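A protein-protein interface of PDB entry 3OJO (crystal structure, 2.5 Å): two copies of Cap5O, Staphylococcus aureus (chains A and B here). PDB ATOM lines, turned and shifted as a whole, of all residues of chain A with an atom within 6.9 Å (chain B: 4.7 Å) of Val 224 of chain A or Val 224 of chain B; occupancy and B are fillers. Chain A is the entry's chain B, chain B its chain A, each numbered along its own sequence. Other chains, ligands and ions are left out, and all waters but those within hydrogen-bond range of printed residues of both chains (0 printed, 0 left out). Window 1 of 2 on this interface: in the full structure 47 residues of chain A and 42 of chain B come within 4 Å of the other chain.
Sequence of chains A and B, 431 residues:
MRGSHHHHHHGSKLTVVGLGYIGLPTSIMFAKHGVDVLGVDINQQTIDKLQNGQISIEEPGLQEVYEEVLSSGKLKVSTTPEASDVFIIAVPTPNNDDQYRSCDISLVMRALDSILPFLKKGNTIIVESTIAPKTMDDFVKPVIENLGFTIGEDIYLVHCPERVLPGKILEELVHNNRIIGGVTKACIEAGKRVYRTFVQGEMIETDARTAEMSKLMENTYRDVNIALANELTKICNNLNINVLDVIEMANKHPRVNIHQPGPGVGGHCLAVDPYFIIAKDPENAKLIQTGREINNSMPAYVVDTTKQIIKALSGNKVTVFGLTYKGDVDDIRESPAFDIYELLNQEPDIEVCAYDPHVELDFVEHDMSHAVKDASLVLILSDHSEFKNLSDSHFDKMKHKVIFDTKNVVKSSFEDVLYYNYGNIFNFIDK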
ATOM      1  N   ASN A 219      27.104 -19.145 -13.149  1.00  0.00           N
ATOM      2  CA  ASN A 219      25.770 -19.650 -13.402  1.00  0.00           C
ATOM      3  C   ASN A 219      25.201 -19.163 -14.730  1.00  0.00           C
ATOM      4  O   ASN A 219      24.504 -19.919 -15.415  1.00  0.00           O
ATOM      5  CB  ASN A 219      24.854 -19.267 -12.248  1.00  0.00           C
ATOM      6  CG  ASN A 219      25.098 -20.034 -10.973  1.00  0.00           C
ATOM      7  OD1 ASN A 219      26.011 -20.848 -10.880  1.00  0.00           O
ATOM      8  ND2 ASN A 219      24.288 -19.774  -9.943  1.00  0.00           N
ATOM      9  N   THR A 220      25.468 -17.896 -15.056  1.00  0.00           N
ATOM     10  CA  THR A 220      25.050 -17.152 -16.243  1.00  0.00           C
ATOM     11  C   THR A 220      25.770 -17.637 -17.512  1.00  0.00           C
ATOM     12  O   THR A 220      25.105 -17.869 -18.529  1.00  0.00           O
ATOM     13  CB  THR A 220      25.237 -15.670 -15.966  1.00  0.00           C
ATOM     14  OG1 THR A 220      24.402 -15.335 -14.859  1.00  0.00           O
ATOM     15  CG2 THR A 220      24.879 -14.818 -17.136  1.00  0.00           C
ATOM     16  N   TYR A 221      27.112 -17.808 -17.450  1.00  0.00           N
ATOM     17  CA  TYR A 221      27.873 -18.343 -18.566  1.00  0.00           C
ATOM     18  C   TYR A 221      27.290 -19.687 -18.937  1.00  0.00           C
ATOM     19  O   TYR A 221      27.084 -19.973 -20.112  1.00  0.00           O
ATOM     20  CB  TYR A 221      29.374 -18.492 -18.231  1.00  0.00           C
ATOM     21  CG  TYR A 221      30.152 -19.269 -19.278  1.00  0.00           C
ATOM     22  CD1 TYR A 221      30.615 -18.649 -20.435  1.00  0.00           C
ATOM     23  CD2 TYR A 221      30.399 -20.628 -19.124  1.00  0.00           C
ATOM     24  CE1 TYR A 221      31.324 -19.368 -21.405  1.00  0.00           C
ATOM     25  CE2 TYR A 221      31.100 -21.351 -20.080  1.00  0.00           C
ATOM     26  CZ  TYR A 221      31.545 -20.725 -21.229  1.00  0.00           C
ATOM     27  OH  TYR A 221      32.230 -21.449 -22.172  1.00  0.00           O
ATOM     28  N   ARG A 222      27.008 -20.504 -17.921  1.00  0.00           N
ATOM     29  CA  ARG A 222      26.439 -21.835 -18.095  1.00  0.00           C
ATOM     30  C   ARG A 222      25.010 -21.797 -18.667  1.00  0.00           C
ATOM     31  O   ARG A 222      24.713 -22.601 -19.525  1.00  0.00           O
ATOM     32  CB  ARG A 222      26.540 -22.624 -16.779  1.00  0.00           C
ATOM     33  CG  ARG A 222      25.958 -24.024 -16.869  1.00  0.00           C
ATOM     34  CD  ARG A 222      25.970 -24.776 -15.553  1.00  0.00           C
ATOM     35  NE  ARG A 222      25.132 -25.978 -15.614  1.00  0.00           N
ATOM     36  CZ  ARG A 222      25.435 -27.105 -16.265  1.00  0.00           C
ATOM     37  NH1 ARG A 222      26.580 -27.208 -16.939  1.00  0.00           N
ATOM     38  NH2 ARG A 222      24.588 -28.126 -16.266  1.00  0.00           N
ATOM     39  N   ASP A 223      24.152 -20.855 -18.229  1.00  0.00           N
ATOM     40  CA  ASP A 223      22.765 -20.774 -18.680  1.00  0.00           C
ATOM     41  C   ASP A 223      22.640 -20.290 -20.113  1.00  0.00           C
ATOM     42  O   ASP A 223      21.904 -20.891 -20.883  1.00  0.00           O
ATOM     43  CB  ASP A 223      21.910 -19.928 -17.707  1.00  0.00           C
ATOM     44  CG  ASP A 223      20.407 -20.089 -17.882  1.00  0.00           C
ATOM     45  OD1 ASP A 223      19.872 -21.126 -17.471  1.00  0.00           O
ATOM     46  OD2 ASP A 223      19.771 -19.168 -18.410  1.00  0.00           O
ATOM     47  N   VAL A 224      23.366 -19.214 -20.466  1.00  0.00           N
ATOM     48  CA  VAL A 224      23.405 -18.605 -21.784  1.00  0.00           C
ATOM     49  C   VAL A 224      23.961 -19.627 -22.810  1.00  0.00           C
ATOM     50  O   VAL A 224      23.453 -19.718 -23.947  1.00  0.00           O
ATOM     51  CB  VAL A 224      24.209 -17.271 -21.745  1.00  0.00           C
ATOM     52  CG1 VAL A 224      24.473 -16.740 -23.163  1.00  0.00           C
ATOM     53  CG2 VAL A 224      23.505 -16.190 -20.894  1.00  0.00           C
ATOM     54  N   ASN A 225      24.997 -20.400 -22.397  1.00  0.00           N
ATOM     55  CA  ASN A 225      25.612 -21.398 -23.264  1.00  0.00           C
ATOM     56  C   ASN A 225      24.727 -22.639 -23.504  1.00  0.00           C
ATOM     57  O   ASN A 225      24.701 -23.186 -24.619  1.00  0.00           O
ATOM     58  CB  ASN A 225      27.018 -21.723 -22.816  1.00  0.00           C
ATOM     59  CG  ASN A 225      27.993 -20.730 -23.362  1.00  0.00           C
ATOM     60  OD1 ASN A 225      28.356 -19.755 -22.707  1.00  0.00           O
ATOM     61  ND2 ASN A 225      28.328 -20.877 -24.627  1.00  0.00           N
ATOM     62  N   ILE A 226      23.958 -23.025 -22.478  1.00  0.00           N
ATOM     63  CA  ILE A 226      22.993 -24.108 -22.570  1.00  0.00           C
ATOM     64  C   ILE A 226      21.860 -23.643 -23.495  1.00  0.00           C
ATOM     65  O   ILE A 226      21.465 -24.400 -24.371  1.00  0.00           O
ATOM     66  CB  ILE A 226      22.513 -24.604 -21.184  1.00  0.00           C
ATOM     67  CG1 ILE A 226      23.663 -25.377 -20.467  1.00  0.00           C
ATOM     68  CG2 ILE A 226      21.254 -25.478 -21.330  1.00  0.00           C
ATOM     69  CD1 ILE A 226      23.307 -25.852 -18.976  1.00  0.00           C
ATOM     70  N   ALA A 227      21.394 -22.379 -23.343  1.00  0.00           N
ATOM     71  CA  ALA A 227      20.379 -21.752 -24.211  1.00  0.00           C
ATOM     72  C   ALA A 227      20.854 -21.794 -25.679  1.00  0.00           C
ATOM     73  O   ALA A 227      20.077 -22.151 -26.564  1.00  0.00           O
ATOM     74  CB  ALA A 227      20.141 -20.313 -23.778  1.00  0.00           C
ATOM     75  N   LEU A 228      22.136 -21.484 -25.918  1.00  0.00           N
ATOM     76  CA  LEU A 228      22.733 -21.541 -27.254  1.00  0.00           C
ATOM     77  C   LEU A 228      22.637 -22.940 -27.876  1.00  0.00           C
ATOM     78  O   LEU A 228      22.200 -23.074 -29.010  1.00  0.00           O
ATOM     79  CB  LEU A 228      24.173 -21.006 -27.229  1.00  0.00           C
ATOM     80  CG  LEU A 228      24.966 -21.092 -28.551  1.00  0.00           C
ATOM     81  CD1 LEU A 228      24.228 -20.402 -29.684  1.00  0.00           C
ATOM     82  CD2 LEU A 228      26.316 -20.503 -28.381  1.00  0.00           C
ATOM     83  N   ALA A 229      23.004 -23.966 -27.105  1.00  0.00           N
ATOM     84  CA  ALA A 229      22.946 -25.378 -27.465  1.00  0.00           C
ATOM     85  C   ALA A 229      21.512 -25.788 -27.778  1.00  0.00           C
ATOM     86  O   ALA A 229      21.268 -26.394 -28.818  1.00  0.00           O
ATOM     87  CB  ALA A 229      23.507 -26.218 -26.330  1.00  0.00           C
ATOM     88  N   GLU A 231      18.890 -23.757 -28.523  1.00  0.00           N
ATOM     89  CA  GLU A 231      18.412 -23.010 -29.681  1.00  0.00           C
ATOM     90  C   GLU A 231      18.929 -23.669 -30.983  1.00  0.00           C
ATOM     91  O   GLU A 231      18.192 -23.789 -31.973  1.00  0.00           O
ATOM     92  CB  GLU A 231      18.864 -21.546 -29.577  1.00  0.00           C
ATOM     93  CG  GLU A 231      18.534 -20.712 -30.800  1.00  0.00           C
ATOM     94  CD  GLU A 231      18.661 -19.221 -30.594  1.00  0.00           C
ATOM     95  OE1 GLU A 231      17.722 -18.618 -30.028  1.00  0.00           O
ATOM     96  OE2 GLU A 231      19.679 -18.646 -31.041  1.00  0.00           O
ATOM     97  N   HIS A 259      28.008 -26.018 -25.331  1.00  0.00           N
ATOM     98  CA  HIS A 259      27.490 -26.919 -24.315  1.00  0.00           C
ATOM     99  C   HIS A 259      26.541 -27.972 -24.886  1.00  0.00           C
ATOM    100  O   HIS A 259      26.245 -27.981 -26.078  1.00  0.00           O
ATOM    101  CB  HIS A 259      26.866 -26.121 -23.138  1.00  0.00           C
ATOM    102  CG  HIS A 259      27.836 -25.231 -22.408  1.00  0.00           C
ATOM    103  ND1 HIS A 259      27.610 -24.847 -21.087  1.00  0.00           N
ATOM    104  CD2 HIS A 259      29.007 -24.683 -22.826  1.00  0.00           C
ATOM    105  CE1 HIS A 259      28.644 -24.083 -20.759  1.00  0.00           C
ATOM    106  NE2 HIS A 259      29.499 -23.939 -21.781  1.00  0.00           N
ATOM    107  N   LEU A 270      20.567 -16.708 -11.248  1.00  0.00           N
ATOM    108  CA  LEU A 270      21.524 -15.925 -12.039  1.00  0.00           C
ATOM    109  C   LEU A 270      22.003 -14.557 -11.527  1.00  0.00           C
ATOM    110  O   LEU A 270      21.503 -14.072 -10.510  1.00  0.00           O
ATOM    111  CB  LEU A 270      21.048 -15.827 -13.495  1.00  0.00           C
ATOM    112  CG  LEU A 270      20.601 -17.093 -14.179  1.00  0.00           C
ATOM    113  CD1 LEU A 270      20.241 -16.801 -15.608  1.00  0.00           C
ATOM    114  CD2 LEU A 270      21.663 -18.193 -14.109  1.00  0.00           C
ATOM    115  N   LEU A 287      20.409 -10.442 -23.094  1.00  0.00           N
ATOM    116  CA  LEU A 287      20.950 -11.773 -23.415  1.00  0.00           C
ATOM    117  C   LEU A 287      20.584 -12.790 -22.375  1.00  0.00           C
ATOM    118  O   LEU A 287      20.196 -13.903 -22.725  1.00  0.00           O
ATOM    119  CB  LEU A 287      22.482 -11.744 -23.565  1.00  0.00           C
ATOM    120  CG  LEU A 287      23.131 -12.940 -24.280  1.00  0.00           C
ATOM    121  CD1 LEU A 287      22.848 -12.918 -25.779  1.00  0.00           C
ATOM    122  CD2 LEU A 287      24.599 -12.898 -24.108  1.00  0.00           C
ATOM    123  N   ILE A 288      20.735 -12.419 -21.081  1.00  0.00           N
ATOM    124  CA  ILE A 288      20.396 -13.284 -19.948  1.00  0.00           C
ATOM    125  C   ILE A 288      18.907 -13.671 -20.006  1.00  0.00           C
ATOM    126  O   ILE A 288      18.589 -14.845 -19.858  1.00  0.00           O
ATOM    127  CB  ILE A 288      20.835 -12.675 -18.581  1.00  0.00           C
ATOM    128  CG1 ILE A 288      22.369 -12.516 -18.535  1.00  0.00           C
ATOM    129  CG2 ILE A 288      20.346 -13.544 -17.400  1.00  0.00           C
ATOM    130  CD1 ILE A 288      22.905 -11.480 -17.563  1.00  0.00           C
ATOM    131  N   GLN A 289      18.024 -12.689 -20.250  1.00  0.00           N
ATOM    132  CA  GLN A 289      16.571 -12.864 -20.367  1.00  0.00           C
ATOM    133  C   GLN A 289      16.217 -13.852 -21.491  1.00  0.00           C
ATOM    134  O   GLN A 289      15.457 -14.796 -21.267  1.00  0.00           O
ATOM    135  CB  GLN A 289      15.923 -11.501 -20.635  1.00  0.00           C
ATOM    136  CG  GLN A 289      14.399 -11.489 -20.633  1.00  0.00           C
ATOM    137  CD  GLN A 289      13.891 -10.134 -21.056  1.00  0.00           C
ATOM    138  OE1 GLN A 289      14.148  -9.662 -22.174  1.00  0.00           O
ATOM    139  NE2 GLN A 289      13.158  -9.480 -20.167  1.00  0.00           N
ATOM    140  N   GLY A 291      18.211 -16.065 -22.945  1.00  0.00           N
ATOM    141  CA  GLY A 291      18.745 -17.361 -22.546  1.00  0.00           C
ATOM    142  C   GLY A 291      17.797 -18.136 -21.652  1.00  0.00           C
ATOM    143  O   GLY A 291      17.639 -19.340 -21.805  1.00  0.00           O
ATOM    144  N   ARG A 292      17.164 -17.434 -20.720  1.00  0.00           N
ATOM    145  CA  ARG A 292      16.189 -17.942 -19.754  1.00  0.00           C
ATOM    146  C   ARG A 292      14.887 -18.347 -20.473  1.00  0.00           C
ATOM    147  O   ARG A 292      14.333 -19.419 -20.203  1.00  0.00           O
ATOM    148  CB  ARG A 292      15.906 -16.864 -18.690  1.00  0.00           C
ATOM    149  CG  ARG A 292      16.953 -16.776 -17.580  1.00  0.00           C
ATOM    150  CD  ARG A 292      16.612 -17.665 -16.401  1.00  0.00           C
ATOM    151  NE  ARG A 292      16.980 -19.071 -16.629  1.00  0.00           N
ATOM    152  CZ  ARG A 292      16.112 -20.063 -16.825  1.00  0.00           C
ATOM    153  NH1 ARG A 292      14.806 -19.828 -16.801  1.00  0.00           N
ATOM    154  NH2 ARG A 292      16.545 -21.296 -17.048  1.00  0.00           N
ATOM    155  N   ILE A 294      14.602 -19.247 -23.673  1.00  0.00           N
ATOM    156  CA  ILE A 294      14.934 -20.437 -24.461  1.00  0.00           C
ATOM    157  C   ILE A 294      14.934 -21.656 -23.570  1.00  0.00           C
ATOM    158  O   ILE A 294      14.279 -22.639 -23.901  1.00  0.00           O
ATOM    159  CB  ILE A 294      16.241 -20.279 -25.313  1.00  0.00           C
ATOM    160  CG1 ILE A 294      16.100 -19.153 -26.357  1.00  0.00           C
ATOM    161  CG2 ILE A 294      16.628 -21.578 -26.014  1.00  0.00           C
ATOM    162  CD1 ILE A 294      17.370 -18.444 -26.658  1.00  0.00           C
ATOM    163  N   ASN A 295      15.592 -21.568 -22.405  1.00  0.00           N
ATOM    164  CA  ASN A 295      15.648 -22.667 -21.440  1.00  0.00           C
ATOM    165  C   ASN A 295      14.290 -23.044 -20.851  1.00  0.00           C
ATOM    166  O   ASN A 295      14.019 -24.239 -20.652  1.00  0.00           O
ATOM    167  CB  ASN A 295      16.727 -22.449 -20.377  1.00  0.00           C
ATOM    168  CG  ASN A 295      18.127 -22.464 -20.948  1.00  0.00           C
ATOM    169  OD1 ASN A 295      18.407 -23.074 -21.984  1.00  0.00           O
ATOM    170  ND2 ASN A 295      19.045 -21.784 -20.297  1.00  0.00           N
ATOM    171  N   THR B 220      28.836 -18.227 -33.750  1.00  0.00           N
ATOM    172  CA  THR B 220      27.726 -18.089 -32.821  1.00  0.00           C
ATOM    173  C   THR B 220      28.213 -18.229 -31.367  1.00  0.00           C
ATOM    174  O   THR B 220      27.893 -17.356 -30.563  1.00  0.00           O
ATOM    175  CB  THR B 220      26.656 -19.089 -33.203  1.00  0.00           C
ATOM    176  OG1 THR B 220      26.117 -18.663 -34.438  1.00  0.00           O
ATOM    177  CG2 THR B 220      25.570 -19.198 -32.210  1.00  0.00           C
ATOM    178  N   TYR B 221      28.973 -19.307 -31.025  1.00  0.00           N
ATOM    179  CA  TYR B 221      29.521 -19.473 -29.687  1.00  0.00           C
ATOM    180  C   TYR B 221      30.336 -18.240 -29.321  1.00  0.00           C
ATOM    181  O   TYR B 221      30.191 -17.708 -28.217  1.00  0.00           O
ATOM    182  CB  TYR B 221      30.401 -20.730 -29.571  1.00  0.00           C
ATOM    183  CG  TYR B 221      31.125 -20.814 -28.230  1.00  0.00           C
ATOM    184  CD1 TYR B 221      30.482 -21.307 -27.095  1.00  0.00           C
ATOM    185  CD2 TYR B 221      32.439 -20.368 -28.091  1.00  0.00           C
ATOM    186  CE1 TYR B 221      31.132 -21.364 -25.864  1.00  0.00           C
ATOM    187  CE2 TYR B 221      33.097 -20.429 -26.871  1.00  0.00           C
ATOM    188  CZ  TYR B 221      32.438 -20.920 -25.757  1.00  0.00           C
ATOM    189  OH  TYR B 221      33.095 -20.986 -24.557  1.00  0.00           O
ATOM    190  N   ARG B 222      31.193 -17.808 -30.241  1.00  0.00           N
ATOM    191  CA  ARG B 222      32.063 -16.648 -30.084  1.00  0.00           C
ATOM    192  C   ARG B 222      31.264 -15.341 -29.870  1.00  0.00           C
ATOM    193  O   ARG B 222      31.474 -14.656 -28.863  1.00  0.00           O
ATOM    194  CB  ARG B 222      33.066 -16.578 -31.267  1.00  0.00           C
ATOM    195  CG  ARG B 222      34.187 -15.564 -31.090  1.00  0.00           C
ATOM    196  CD  ARG B 222      33.935 -14.319 -31.909  1.00  0.00           C
ATOM    197  NE  ARG B 222      34.584 -14.393 -33.215  1.00  0.00           N
ATOM    198  CZ  ARG B 222      33.948 -14.456 -34.380  1.00  0.00           C
ATOM    199  NH1 ARG B 222      32.621 -14.451 -34.424  1.00  0.00           N
ATOM    200  NH2 ARG B 222      34.633 -14.521 -35.514  1.00  0.00           N
ATOM    201  N   ASP B 223      30.341 -15.019 -30.781  1.00  0.00           N
ATOM    202  CA  ASP B 223      29.521 -13.807 -30.684  1.00  0.00           C
ATOM    203  C   ASP B 223      28.612 -13.706 -29.462  1.00  0.00           C
ATOM    204  O   ASP B 223      28.538 -12.637 -28.860  1.00  0.00           O
ATOM    205  CB  ASP B 223      28.715 -13.575 -31.968  1.00  0.00           C
ATOM    206  CG  ASP B 223      29.555 -13.137 -33.161  1.00  0.00           C
ATOM    207  OD1 ASP B 223      30.791 -12.949 -32.988  1.00  0.00           O
ATOM    208  OD2 ASP B 223      28.985 -13.003 -34.266  1.00  0.00           O
ATOM    209  N   VAL B 224      27.914 -14.802 -29.116  1.00  0.00           N
ATOM    210  CA  VAL B 224      27.016 -14.877 -27.964  1.00  0.00           C
ATOM    211  C   VAL B 224      27.853 -14.669 -26.687  1.00  0.00           C
ATOM    212  O   VAL B 224      27.406 -13.968 -25.776  1.00  0.00           O
ATOM    213  CB  VAL B 224      26.174 -16.206 -27.929  1.00  0.00           C
ATOM    214  CG1 VAL B 224      25.414 -16.385 -26.617  1.00  0.00           C
ATOM    215  CG2 VAL B 224      25.203 -16.284 -29.109  1.00  0.00           C
ATOM    216  N   ASN B 225      29.063 -15.272 -26.631  1.00  0.00           N
ATOM    217  CA  ASN B 225      29.928 -15.152 -25.474  1.00  0.00           C
ATOM    218  C   ASN B 225      30.551 -13.763 -25.289  1.00  0.00           C
ATOM    219  O   ASN B 225      30.672 -13.272 -24.143  1.00  0.00           O
ATOM    220  CB  ASN B 225      30.920 -16.293 -25.410  1.00  0.00           C
ATOM    221  CG  ASN B 225      30.308 -17.507 -24.787  1.00  0.00           C
ATOM    222  OD1 ASN B 225      29.804 -18.399 -25.468  1.00  0.00           O
ATOM    223  ND2 ASN B 225      30.190 -17.490 -23.478  1.00  0.00           N
ATOM    224  N   ILE B 226      30.889 -13.105 -26.417  1.00  0.00           N
ATOM    225  CA  ILE B 226      31.412 -11.736 -26.396  1.00  0.00           C
ATOM    226  C   ILE B 226      30.280 -10.812 -25.958  1.00  0.00           C
ATOM    227  O   ILE B 226      30.489  -9.964 -25.094  1.00  0.00           O
ATOM    228  CB  ILE B 226      32.076 -11.324 -27.727  1.00  0.00           C
ATOM    229  CG1 ILE B 226      33.422 -12.079 -27.894  1.00  0.00           C
ATOM    230  CG2 ILE B 226      32.317  -9.794 -27.752  1.00  0.00           C
ATOM    231  CD1 ILE B 226      34.208 -11.841 -29.232  1.00  0.00           C
ATOM    232  N   ALA B 227      29.058 -11.042 -26.502  1.00  0.00           N
ATOM    233  CA  ALA B 227      27.839 -10.313 -26.133  1.00  0.00           C
ATOM    234  C   ALA B 227      27.592 -10.440 -24.624  1.00  0.00           C
ATOM    235  O   ALA B 227      27.297  -9.443 -23.984  1.00  0.00           O
ATOM    236  CB  ALA B 227      26.658 -10.870 -26.894  1.00  0.00           C
ATOM    237  N   LEU B 228      27.771 -11.655 -24.052  1.00  0.00           N
ATOM    238  CA  LEU B 228      27.611 -11.911 -22.621  1.00  0.00           C
ATOM    239  C   LEU B 228      28.562 -11.053 -21.793  1.00  0.00           C
ATOM    240  O   LEU B 228      28.116 -10.413 -20.849  1.00  0.00           O
ATOM    241  CB  LEU B 228      27.749 -13.403 -22.305  1.00  0.00           C
ATOM    242  CG  LEU B 228      27.696 -13.812 -20.812  1.00  0.00           C
ATOM    243  CD1 LEU B 228      26.414 -13.320 -20.131  1.00  0.00           C
ATOM    244  CD2 LEU B 228      27.847 -15.307 -20.657  1.00  0.00           C
ATOM    245  N   LEU B 287      18.449 -15.795 -29.509  1.00  0.00           N
ATOM    246  CA  LEU B 287      19.687 -15.589 -28.743  1.00  0.00           C
ATOM    247  C   LEU B 287      20.791 -15.060 -29.616  1.00  0.00           C
ATOM    248  O   LEU B 287      21.498 -14.130 -29.210  1.00  0.00           O
ATOM    249  CB  LEU B 287      20.142 -16.892 -28.038  1.00  0.00           C
ATOM    250  CG  LEU B 287      21.195 -16.757 -26.928  1.00  0.00           C
ATOM    251  CD1 LEU B 287      20.646 -16.065 -25.694  1.00  0.00           C
ATOM    252  CD2 LEU B 287      21.705 -18.074 -26.535  1.00  0.00           C
ATOM    253  N   ILE B 288      20.962 -15.663 -30.802  1.00  0.00           N
ATOM    254  CA  ILE B 288      21.974 -15.258 -31.778  1.00  0.00           C
ATOM    255  C   ILE B 288      21.763 -13.798 -32.202  1.00  0.00           C
ATOM    256  O   ILE B 288      22.719 -13.031 -32.209  1.00  0.00           O
ATOM    257  CB  ILE B 288      22.057 -16.243 -32.989  1.00  0.00           C
ATOM    258  CG1 ILE B 288      22.425 -17.665 -32.503  1.00  0.00           C
ATOM    259  CG2 ILE B 288      23.086 -15.759 -34.005  1.00  0.00           C
ATOM    260  CD1 ILE B 288      22.008 -18.829 -33.457  1.00  0.00           C
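ND2 of Asn 225 of chain A is in hydrogen-bond range of OD1 of Asn 225 of chain B. The side-chain carboxylate of Glu 231 of chain A sits at hydrogen-bond distance from the backbone NH of Leu 287 of chain B, at 3.0 Å. The backbone NH (N) of Ile 288 of chain B sits at hydrogen-bond distance from the side-chain carboxylate (OE2) of Glu 231 of chain A. OH of Tyr 221 of chain A is in hydrogen-bond range of OH of Tyr 221 of chain B (2.6 Å).
Among the printed residues, merely in contact across the chains: Tyr 221 of chain A with Asn 225 of chain B, Asn 225 of chain A with Tyr 221 of chain B, Leu 228 of chain A with Thr 220 of chain B, Leu 287 of chain A with Leu 228 of chain B, Leu 287 of chain A with Val 224 of chain B, Ile 294 of chain A with Leu 287 of chain B, Leu 228 of chain A with Leu 287 of chain B, Val 224 of chain A with Leu 287 of chain B, Val 224 of chain A with Val 224 of chain B, Leu 228 of chain A with Tyr 221 of chain B, Gly 291 of chain A with Leu 287 of chain B, Thr 220 of chain A with Leu 228 of chain B, Tyr 221 of chain A with Leu 228 of chain B, Leu 287 of chain A with Leu 287 of chain B, Ala 227 of chain A with Leu 287 of chain B and Leu 287 of chain A with Ala 227 of chain B.
Hydrophobic or aromatic side chains of chain A within 4 Å of the printed part of chain B: Tyr 221, Val 224, Ala 227, Leu 228, Leu 287 and Ile 294. Of the 11 printed residues of chain B, 8 touch a printed residue of chain A. Hydrophobic or aromatic side chains of chain B that line the printed part of chain A: Tyr 221, Val 224, Leu 228, Leu 287 and Ile 288. Among the printed residues, no Asp or Glu carboxylate lies within 4 Å of a Lys or Arg side-chain nitrogen of the other chain.
Thr 220 of chain A touches Leu 228 of chain B, and with the chains exchanged Leu 228 of chain A touches Thr 220 of chain B. Tyr 221 of chain A touches Leu 228 of chain B, and with the chains exchanged Leu 228 of chain A touches Tyr 221 of chain B. Asn 225 of chain B touches its own counterpart, Asn 225 of chain A. Ala 227 of chain A touches Leu 287 of chain B, and with the chains exchanged Leu 287 of chain A touches Ala 227 of chain B. Positions printed for both chains: 220, 221, 222, 223, 224, 225, 226, 227, 228, 287 and 288. Of the 20 pairs that touch across the chains among the printed residues, 16 have their exchanged pair printed and touching as well.
The side-chain amide oxygen (OD1) of Asn 225 of chain B lies close to the backbone carbonyl oxygen (O) of Tyr 221 of chain B, 2.9 Å away. O of Tyr 221 of chain A sits close to OD1 of Asn 225 of chain A, 2.9 Å away. The side-chain amide nitrogen (ND2) of Asn 295 of chain A is in hydrogen-bond range of the backbone carbonyl oxygen (O) of Gly 291 of chain A (3.2 Å). The side-chain amide oxygen (OD1) of Asn 295 of chain A sits close to the backbone NH (N) of Ala 227 of chain A (3.4 Å).
Val 224 of chain A touches two residues of chain B. Leu 270 of chain A touches none of the printed residues of chain B. Of the printed residues of chain B, Leu 287 of chain A touches Val 224, Ala 227, Leu 228 and Leu 287. Printed residues of chain B within 4 Å of Ile 294 of chain A: Leu 287. Of the printed residues of chain A, Thr 220 of chain B touches Leu 228. Val 224 of chain B touches two residues of chain A. Of the printed residues of chain A, Asn 225 of chain B touches Tyr 221 (3.0 Å) and Asn 225 (3.0 Å). The nearest residue of chain B that does not touch Val 224 of chain A is Leu 228 of chain B (4.2 Å). The nearest residue of chain A that does not touch Val 224 of chain B is Leu 228 of chain A (4.3 Å).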
